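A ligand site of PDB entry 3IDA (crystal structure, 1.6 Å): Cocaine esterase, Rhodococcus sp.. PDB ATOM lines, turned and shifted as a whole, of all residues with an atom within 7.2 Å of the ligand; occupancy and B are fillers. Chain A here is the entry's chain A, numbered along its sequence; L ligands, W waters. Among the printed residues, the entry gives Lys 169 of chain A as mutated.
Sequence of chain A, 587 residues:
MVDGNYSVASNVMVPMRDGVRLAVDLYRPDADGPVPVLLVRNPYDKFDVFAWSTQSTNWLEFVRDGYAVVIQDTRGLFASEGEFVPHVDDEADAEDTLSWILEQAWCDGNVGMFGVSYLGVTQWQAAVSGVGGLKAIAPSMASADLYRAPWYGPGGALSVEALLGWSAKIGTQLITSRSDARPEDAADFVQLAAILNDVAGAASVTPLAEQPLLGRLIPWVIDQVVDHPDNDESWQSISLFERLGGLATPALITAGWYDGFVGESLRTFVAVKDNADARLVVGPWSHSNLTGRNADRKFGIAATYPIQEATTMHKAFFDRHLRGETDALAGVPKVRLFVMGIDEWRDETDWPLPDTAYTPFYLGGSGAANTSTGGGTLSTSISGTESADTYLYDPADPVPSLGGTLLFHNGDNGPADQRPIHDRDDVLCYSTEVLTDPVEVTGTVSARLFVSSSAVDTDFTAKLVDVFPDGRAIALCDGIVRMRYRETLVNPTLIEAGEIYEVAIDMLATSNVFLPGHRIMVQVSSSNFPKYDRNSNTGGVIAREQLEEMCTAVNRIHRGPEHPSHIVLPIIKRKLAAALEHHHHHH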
ATOM      1  N   PRO A  43      19.803  -1.980  25.783  1.00  0.00           N
ATOM      2  CA  PRO A  43      19.438  -2.236  27.180  1.00  0.00           C
ATOM      3  C   PRO A  43      20.223  -3.364  27.886  1.00  0.00           C
ATOM      4  O   PRO A  43      19.874  -3.752  29.023  1.00  0.00           O
ATOM      5  CB  PRO A  43      17.963  -2.628  27.079  1.00  0.00           C
ATOM      6  CG  PRO A  43      17.888  -3.380  25.768  1.00  0.00           C
ATOM      7  CD  PRO A  43      18.964  -2.779  24.854  1.00  0.00           C
ATOM      8  N   TYR A  44      21.256  -3.897  27.236  1.00  0.00           N
ATOM      9  CA  TYR A  44      21.990  -5.080  27.732  1.00  0.00           C
ATOM     10  C   TYR A  44      23.484  -4.802  28.060  1.00  0.00           C
ATOM     11  O   TYR A  44      24.324  -5.699  27.952  1.00  0.00           O
ATOM     12  CB  TYR A  44      21.856  -6.256  26.748  1.00  0.00           C
ATOM     13  CG  TYR A  44      20.448  -6.560  26.222  1.00  0.00           C
ATOM     14  CD1 TYR A  44      19.439  -7.042  27.061  1.00  0.00           C
ATOM     15  CD2 TYR A  44      20.131  -6.381  24.859  1.00  0.00           C
ATOM     16  CE1 TYR A  44      18.151  -7.327  26.573  1.00  0.00           C
ATOM     17  CE2 TYR A  44      18.855  -6.666  24.362  1.00  0.00           C
ATOM     18  CZ  TYR A  44      17.870  -7.150  25.219  1.00  0.00           C
ATOM     19  OH  TYR A  44      16.609  -7.428  24.718  1.00  0.00           O
ATOM     20  N   HIS A  87      10.056   0.458  26.363  1.00  0.00           N
ATOM     21  CA  HIS A  87       9.426   1.186  25.235  1.00  0.00           C
ATOM     22  C   HIS A  87       9.017   2.672  25.430  1.00  0.00           C
ATOM     23  O   HIS A  87       9.158   3.479  24.491  1.00  0.00           O
ATOM     24  CB  HIS A  87       8.237   0.411  24.616  1.00  0.00           C
ATOM     25  CG  HIS A  87       8.466  -1.061  24.411  1.00  0.00           C
ATOM     26  ND1 HIS A  87       9.557  -1.574  23.742  1.00  0.00           N
ATOM     27  CD2 HIS A  87       7.712  -2.135  24.762  1.00  0.00           C
ATOM     28  CE1 HIS A  87       9.480  -2.893  23.710  1.00  0.00           C
ATOM     29  NE2 HIS A  87       8.362  -3.257  24.321  1.00  0.00           N
ATOM     30  N   VAL A 116      20.241  -5.084  16.195  1.00  0.00           N
ATOM     31  CA  VAL A 116      19.297  -6.225  16.166  1.00  0.00           C
ATOM     32  C   VAL A 116      18.325  -6.257  17.371  1.00  0.00           C
ATOM     33  O   VAL A 116      18.692  -5.826  18.474  1.00  0.00           O
ATOM     34  CB  VAL A 116      20.110  -7.569  16.086  1.00  0.00           C
ATOM     35  CG1 VAL A 116      20.874  -7.836  17.398  1.00  0.00           C
ATOM     36  CG2 VAL A 116      19.217  -8.754  15.716  1.00  0.00           C
ATOM     37  N   SER A 117      17.096  -6.748  17.150  1.00  0.00           N
ATOM     38  CA  SER A 117      16.108  -6.980  18.237  1.00  0.00           C
ATOM     39  C   SER A 117      15.692  -5.646  18.920  1.00  0.00           C
ATOM     40  O   SER A 117      15.165  -4.770  18.234  1.00  0.00           O
ATOM     41  CB  SER A 117      16.646  -8.049  19.233  1.00  0.00           C
ATOM     42  OG  SER A 117      15.612  -8.677  19.985  1.00  0.00           O
ATOM     43  N   TYR A 118      15.926  -5.476  20.232  1.00  0.00           N
ATOM     44  CA  TYR A 118      15.583  -4.194  20.918  1.00  0.00           C
ATOM     45  C   TYR A 118      16.413  -3.041  20.321  1.00  0.00           C
ATOM     46  O   TYR A 118      15.944  -1.888  20.278  1.00  0.00           O
ATOM     47  CB  TYR A 118      15.809  -4.310  22.438  1.00  0.00           C
ATOM     48  CG  TYR A 118      15.063  -3.309  23.348  1.00  0.00           C
ATOM     49  CD1 TYR A 118      15.511  -1.997  23.527  1.00  0.00           C
ATOM     50  CD2 TYR A 118      13.939  -3.717  24.088  1.00  0.00           C
ATOM     51  CE1 TYR A 118      14.848  -1.105  24.394  1.00  0.00           C
ATOM     52  CE2 TYR A 118      13.271  -2.831  24.950  1.00  0.00           C
ATOM     53  CZ  TYR A 118      13.723  -1.528  25.100  1.00  0.00           C
ATOM     54  OH  TYR A 118      13.072  -0.653  25.960  1.00  0.00           O
ATOM     55  N   LEU A 119      17.614  -3.362  19.844  1.00  0.00           N
ATOM     56  CA  LEU A 119      18.512  -2.397  19.188  1.00  0.00           C
ATOM     57  C   LEU A 119      18.011  -2.034  17.773  1.00  0.00           C
ATOM     58  O   LEU A 119      18.545  -1.124  17.129  1.00  0.00           O
ATOM     59  CB  LEU A 119      19.949  -2.941  19.118  1.00  0.00           C
ATOM     60  CG  LEU A 119      20.788  -3.141  20.396  1.00  0.00           C
ATOM     61  CD1 LEU A 119      20.148  -4.081  21.428  1.00  0.00           C
ATOM     62  CD2 LEU A 119      22.171  -3.658  20.022  1.00  0.00           C
ATOM     63  N   GLY A 120      16.997  -2.773  17.304  1.00  0.00           N
ATOM     64  CA  GLY A 120      16.289  -2.497  16.040  1.00  0.00           C
ATOM     65  C   GLY A 120      14.986  -1.732  16.228  1.00  0.00           C
ATOM     66  O   GLY A 120      14.707  -0.773  15.487  1.00  0.00           O
ATOM     67  N   VAL A 121      14.169  -2.150  17.203  1.00  0.00           N
ATOM     68  CA  VAL A 121      12.936  -1.429  17.580  1.00  0.00           C
ATOM     69  C   VAL A 121      13.211   0.069  17.835  1.00  0.00           C
ATOM     70  O   VAL A 121      12.475   0.940  17.362  1.00  0.00           O
ATOM     71  CB  VAL A 121      12.234  -2.077  18.824  1.00  0.00           C
ATOM     72  CG1 VAL A 121      11.049  -1.219  19.315  1.00  0.00           C
ATOM     73  CG2 VAL A 121      11.779  -3.519  18.526  1.00  0.00           C
ATOM     74  N   MET A 141      15.732  -7.980  12.558  1.00  0.00           N
ATOM     75  CA  MET A 141      14.881  -8.835  13.395  1.00  0.00           C
ATOM     76  C   MET A 141      14.068  -7.995  14.414  1.00  0.00           C
ATOM     77  O   MET A 141      14.152  -8.207  15.637  1.00  0.00           O
ATOM     78  CB  MET A 141      15.703  -9.971  14.045  1.00  0.00           C
ATOM     79  CG  MET A 141      16.376 -10.922  13.011  1.00  0.00           C
ATOM     80  SD  MET A 141      17.506 -12.206  13.639  1.00  0.00           S
ATOM     81  CE  MET A 141      17.600 -13.283  12.225  1.00  0.00           C
ATOM     82  N   LEU A 146       4.364  -3.036  18.598  1.00  0.00           N
ATOM     83  CA  LEU A 146       4.743  -3.955  19.687  1.00  0.00           C
ATOM     84  C   LEU A 146       3.643  -4.950  20.104  1.00  0.00           C
ATOM     85  O   LEU A 146       3.955  -6.035  20.618  1.00  0.00           O
ATOM     86  CB  LEU A 146       5.302  -3.188  20.900  1.00  0.00           C
ATOM     87  CG  LEU A 146       6.701  -2.536  20.824  1.00  0.00           C
ATOM     88  CD1 LEU A 146       7.795  -3.524  20.334  1.00  0.00           C
ATOM     89  CD2 LEU A 146       6.707  -1.257  19.993  1.00  0.00           C
ATOM     90  N   ALA A 149       4.042  -7.686  17.221  1.00  0.00           N
ATOM     91  CA  ALA A 149       5.250  -8.465  17.568  1.00  0.00           C
ATOM     92  C   ALA A 149       6.155  -7.655  18.499  1.00  0.00           C
ATOM     93  O   ALA A 149       6.447  -6.495  18.194  1.00  0.00           O
ATOM     94  CB  ALA A 149       6.028  -8.873  16.308  1.00  0.00           C
ATOM     95  N   PRO A 150       6.669  -8.261  19.594  1.00  0.00           N
ATOM     96  CA  PRO A 150       6.575  -9.683  19.980  1.00  0.00           C
ATOM     97  C   PRO A 150       5.550 -10.088  21.057  1.00  0.00           C
ATOM     98  O   PRO A 150       5.527 -11.279  21.426  1.00  0.00           O
ATOM     99  CB  PRO A 150       7.988  -9.947  20.529  1.00  0.00           C
ATOM    100  CG  PRO A 150       8.290  -8.642  21.293  1.00  0.00           C
ATOM    101  CD  PRO A 150       7.537  -7.533  20.548  1.00  0.00           C
ATOM    102  N   TRP A 151       4.730  -9.176  21.571  1.00  0.00           N
ATOM    103  CA  TRP A 151       3.949  -9.471  22.793  1.00  0.00           C
ATOM    104  C   TRP A 151       2.584 -10.168  22.595  1.00  0.00           C
ATOM    105  O   TRP A 151       2.251 -11.090  23.354  1.00  0.00           O
ATOM    106  CB  TRP A 151       3.874  -8.246  23.732  1.00  0.00           C
ATOM    107  CG  TRP A 151       5.218  -7.577  24.015  1.00  0.00           C
ATOM    108  CD1 TRP A 151       5.521  -6.248  23.867  1.00  0.00           C
ATOM    109  CD2 TRP A 151       6.432  -8.209  24.480  1.00  0.00           C
ATOM    110  NE1 TRP A 151       6.838  -6.011  24.213  1.00  0.00           N
ATOM    111  CE2 TRP A 151       7.420  -7.196  24.589  1.00  0.00           C
ATOM    112  CE3 TRP A 151       6.787  -9.526  24.813  1.00  0.00           C
ATOM    113  CZ2 TRP A 151       8.732  -7.456  25.024  1.00  0.00           C
ATOM    114  CZ3 TRP A 151       8.093  -9.794  25.242  1.00  0.00           C
ATOM    115  CH2 TRP A 151       9.053  -8.749  25.337  1.00  0.00           C
ATOM    116  N   ALA A 162       7.273 -15.869  25.112  1.00  0.00           N
ATOM    117  CA  ALA A 162       8.133 -14.709  24.834  1.00  0.00           C
ATOM    118  C   ALA A 162       8.166 -13.723  26.023  1.00  0.00           C
ATOM    119  O   ALA A 162       9.248 -13.243  26.412  1.00  0.00           O
ATOM    120  CB  ALA A 162       7.675 -14.007  23.560  1.00  0.00           C
ATOM    121  N   LEU A 163       6.986 -13.433  26.573  1.00  0.00           N
ATOM    122  CA  LEU A 163       6.851 -12.502  27.700  1.00  0.00           C
ATOM    123  C   LEU A 163       7.559 -12.951  28.977  1.00  0.00           C
ATOM    124  O   LEU A 163       8.323 -12.193  29.577  1.00  0.00           O
ATOM    125  CB  LEU A 163       5.373 -12.205  27.992  1.00  0.00           C
ATOM    126  CG  LEU A 163       5.112 -11.215  29.154  1.00  0.00           C
ATOM    127  CD1 LEU A 163       5.615  -9.804  28.814  1.00  0.00           C
ATOM    128  CD2 LEU A 163       3.640 -11.208  29.559  1.00  0.00           C
ATOM    129  N   GLY A 165       9.841 -15.455  29.415  1.00  0.00           N
ATOM    130  CA  GLY A 165      11.276 -15.635  29.158  1.00  0.00           C
ATOM    131  C   GLY A 165      12.071 -14.329  29.147  1.00  0.00           C
ATOM    132  O   GLY A 165      13.099 -14.223  29.834  1.00  0.00           O
ATOM    133  N   TRP A 166      11.610 -13.338  28.394  1.00  0.00           N
ATOM    134  CA  TRP A 166      12.315 -12.038  28.340  1.00  0.00           C
ATOM    135  C   TRP A 166      12.322 -11.327  29.702  1.00  0.00           C
ATOM    136  O   TRP A 166      13.353 -10.779  30.105  1.00  0.00           O
ATOM    137  CB  TRP A 166      11.718 -11.111  27.262  1.00  0.00           C
ATOM    138  CG  TRP A 166      12.563  -9.860  26.976  1.00  0.00           C
ATOM    139  CD1 TRP A 166      13.768  -9.809  26.317  1.00  0.00           C
ATOM    140  CD2 TRP A 166      12.254  -8.504  27.352  1.00  0.00           C
ATOM    141  NE1 TRP A 166      14.226  -8.506  26.250  1.00  0.00           N
ATOM    142  CE2 TRP A 166      13.321  -7.687  26.875  1.00  0.00           C
ATOM    143  CE3 TRP A 166      11.198  -7.899  28.040  1.00  0.00           C
ATOM    144  CZ2 TRP A 166      13.339  -6.292  27.059  1.00  0.00           C
ATOM    145  CZ3 TRP A 166      11.215  -6.504  28.224  1.00  0.00           C
ATOM    146  CH2 TRP A 166      12.283  -5.723  27.737  1.00  0.00           C
ATOM    147  N   LYS A 169      15.003 -12.795  31.849  1.00  0.00           N
ATOM    148  CA  LYS A 169      16.315 -12.345  31.364  1.00  0.00           C
ATOM    149  C   LYS A 169      16.648 -10.941  31.895  1.00  0.00           C
ATOM    150  O   LYS A 169      17.772 -10.710  32.372  1.00  0.00           O
ATOM    151  CB  LYS A 169      16.361 -12.378  29.834  1.00  0.00           C
ATOM    152  CG  LYS A 169      17.650 -11.852  29.206  1.00  0.00           C
ATOM    153  CD  LYS A 169      17.571 -11.876  27.679  1.00  0.00           C
ATOM    154  CE  LYS A 169      18.805 -11.267  27.050  1.00  0.00           C
ATOM    155  NZ  LYS A 169      18.829 -11.516  25.584  1.00  0.00           N
ATOM    156  N   PHE A 261       9.773 -12.078  14.977  1.00  0.00           N
ATOM    157  CA  PHE A 261       9.446 -10.791  14.340  1.00  0.00           C
ATOM    158  C   PHE A 261       9.146 -10.832  12.821  1.00  0.00           C
ATOM    159  O   PHE A 261       8.887  -9.784  12.239  1.00  0.00           O
ATOM    160  CB  PHE A 261      10.567  -9.771  14.580  1.00  0.00           C
ATOM    161  CG  PHE A 261      10.730  -9.331  16.015  1.00  0.00           C
ATOM    162  CD1 PHE A 261      11.558 -10.029  16.893  1.00  0.00           C
ATOM    163  CD2 PHE A 261      10.078  -8.195  16.477  1.00  0.00           C
ATOM    164  CE1 PHE A 261      11.718  -9.601  18.222  1.00  0.00           C
ATOM    165  CE2 PHE A 261      10.220  -7.756  17.807  1.00  0.00           C
ATOM    166  CZ  PHE A 261      11.040  -8.468  18.674  1.00  0.00           C
ATOM    167  N   HIS A 287      15.456 -16.639  16.390  1.00  0.00           N
ATOM    168  CA  HIS A 287      16.045 -15.475  17.105  1.00  0.00           C
ATOM    169  C   HIS A 287      17.386 -15.795  17.780  1.00  0.00           C
ATOM    170  O   HIS A 287      18.282 -14.942  17.822  1.00  0.00           O
ATOM    171  CB  HIS A 287      15.039 -14.889  18.126  1.00  0.00           C
ATOM    172  CG  HIS A 287      15.153 -13.397  18.327  1.00  0.00           C
ATOM    173  ND1 HIS A 287      14.821 -12.492  17.341  1.00  0.00           N
ATOM    174  CD2 HIS A 287      15.482 -12.661  19.413  1.00  0.00           C
ATOM    175  CE1 HIS A 287      14.995 -11.259  17.801  1.00  0.00           C
ATOM    176  NE2 HIS A 287      15.388 -11.339  19.054  1.00  0.00           N
ATOM    177  N   LEU A 407      10.508 -18.177  20.784  1.00  0.00           N
ATOM    178  CA  LEU A 407      11.616 -17.275  21.176  1.00  0.00           C
ATOM    179  C   LEU A 407      12.502 -17.800  22.327  1.00  0.00           C
ATOM    180  O   LEU A 407      13.726 -17.880  22.178  1.00  0.00           O
ATOM    181  CB  LEU A 407      11.088 -15.861  21.485  1.00  0.00           C
ATOM    182  CG  LEU A 407      10.663 -14.985  20.293  1.00  0.00           C
ATOM    183  CD1 LEU A 407       9.773 -13.828  20.696  1.00  0.00           C
ATOM    184  CD2 LEU A 407      11.873 -14.437  19.545  1.00  0.00           C
ATOM    185  N   PHE A 408      11.883 -18.168  23.467  1.00  0.00           N
ATOM    186  CA  PHE A 408      12.593 -18.588  24.690  1.00  0.00           C
ATOM    187  C   PHE A 408      12.374 -20.063  25.102  1.00  0.00           C
ATOM    188  O   PHE A 408      13.295 -20.684  25.654  1.00  0.00           O
ATOM    189  CB  PHE A 408      12.268 -17.647  25.875  1.00  0.00           C
ATOM    190  CG  PHE A 408      12.996 -16.328  25.815  1.00  0.00           C
ATOM    191  CD1 PHE A 408      14.239 -16.171  26.441  1.00  0.00           C
ATOM    192  CD2 PHE A 408      12.450 -15.237  25.135  1.00  0.00           C
ATOM    193  CE1 PHE A 408      14.927 -14.955  26.377  1.00  0.00           C
ATOM    194  CE2 PHE A 408      13.125 -14.022  25.066  1.00  0.00           C
ATOM    195  CZ  PHE A 408      14.371 -13.878  25.686  1.00  0.00           C
HETATM  196  O1  LIG L   1      16.653  -7.839  22.109  1.00  0.00           O
HETATM  197  C1  LIG L   1      15.429  -8.445  21.512  1.00  0.00           C
HETATM  198  O2  LIG L   1      15.012  -9.773  22.138  1.00  0.00           O
HETATM  199  O3  LIG L   1      14.306  -7.579  21.697  1.00  0.00           O
HETATM  200  C2  LIG L   1      13.152  -8.343  22.023  1.00  0.00           C
HETATM  201  C3  LIG L   1      12.223  -7.525  22.932  1.00  0.00           C
HETATM  202  S1  LIG L   1      11.441  -6.093  22.126  1.00  0.00           S
HETATM  203  C4  LIG L   1      13.676  -9.653  22.632  1.00  0.00           C
HETATM  204  C5  LIG L   1      12.914 -10.908  22.221  1.00  0.00           C
HETATM  205  S2  LIG L   1      11.250 -11.099  22.931  1.00  0.00           S
HETATM  206  O   HOH W   1      16.770 -11.326  23.717  1.00  0.00           O
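The side-chain hydroxyl of Ser 117 sits at hydrogen-bond distance from a ring nitrogen (NE2) of His 287. The side-chain hydroxyl (OH) of Tyr 44 is in hydrogen-bond range of the indole nitrogen (NE1) of Trp 166 (3.0 Å). OH of Tyr 118 is in hydrogen-bond range of N of His 87 (3.2 Å).
Water W1 lies within hydrogen-bond range of the side-chain amino group of Lys 169 (2.8 Å) and an oxygen (O2) of the ligand (2.8 Å).
NE2 of His 287 sits at hydrogen-bond distance from O2 of the ligand (3.5 Å). A carbon (C1) of the ligand is covalently linked to the side-chain hydroxyl (OG) of Ser 117 (1.6 Å). An oxygen (O3) of the ligand is in hydrogen-bond range of the backbone NH (N) of Tyr 118 (3.0 Å). An oxygen (O1) of the ligand is in hydrogen-bond range of the side-chain hydroxyl (OH) of Tyr 44, at 2.6 Å.
Merely in contact with the ligand: Trp 166 (3.7 Å), Phe 261 (3.96 Å) and Leu 407 (3.8 Å). Hydrophobic or aromatic side chains that line the ligand: Tyr 44, Tyr 118, Trp 166, Phe 261, His 287 and Leu 407. Seven residues have an atom within 4 Å of the ligand: Tyr 44, Ser 117, Tyr 118, Trp 166, Phe 261, His 287 and Leu 407. Along chain A the residues within 4 Å of the ligand span positions 44 to 407.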
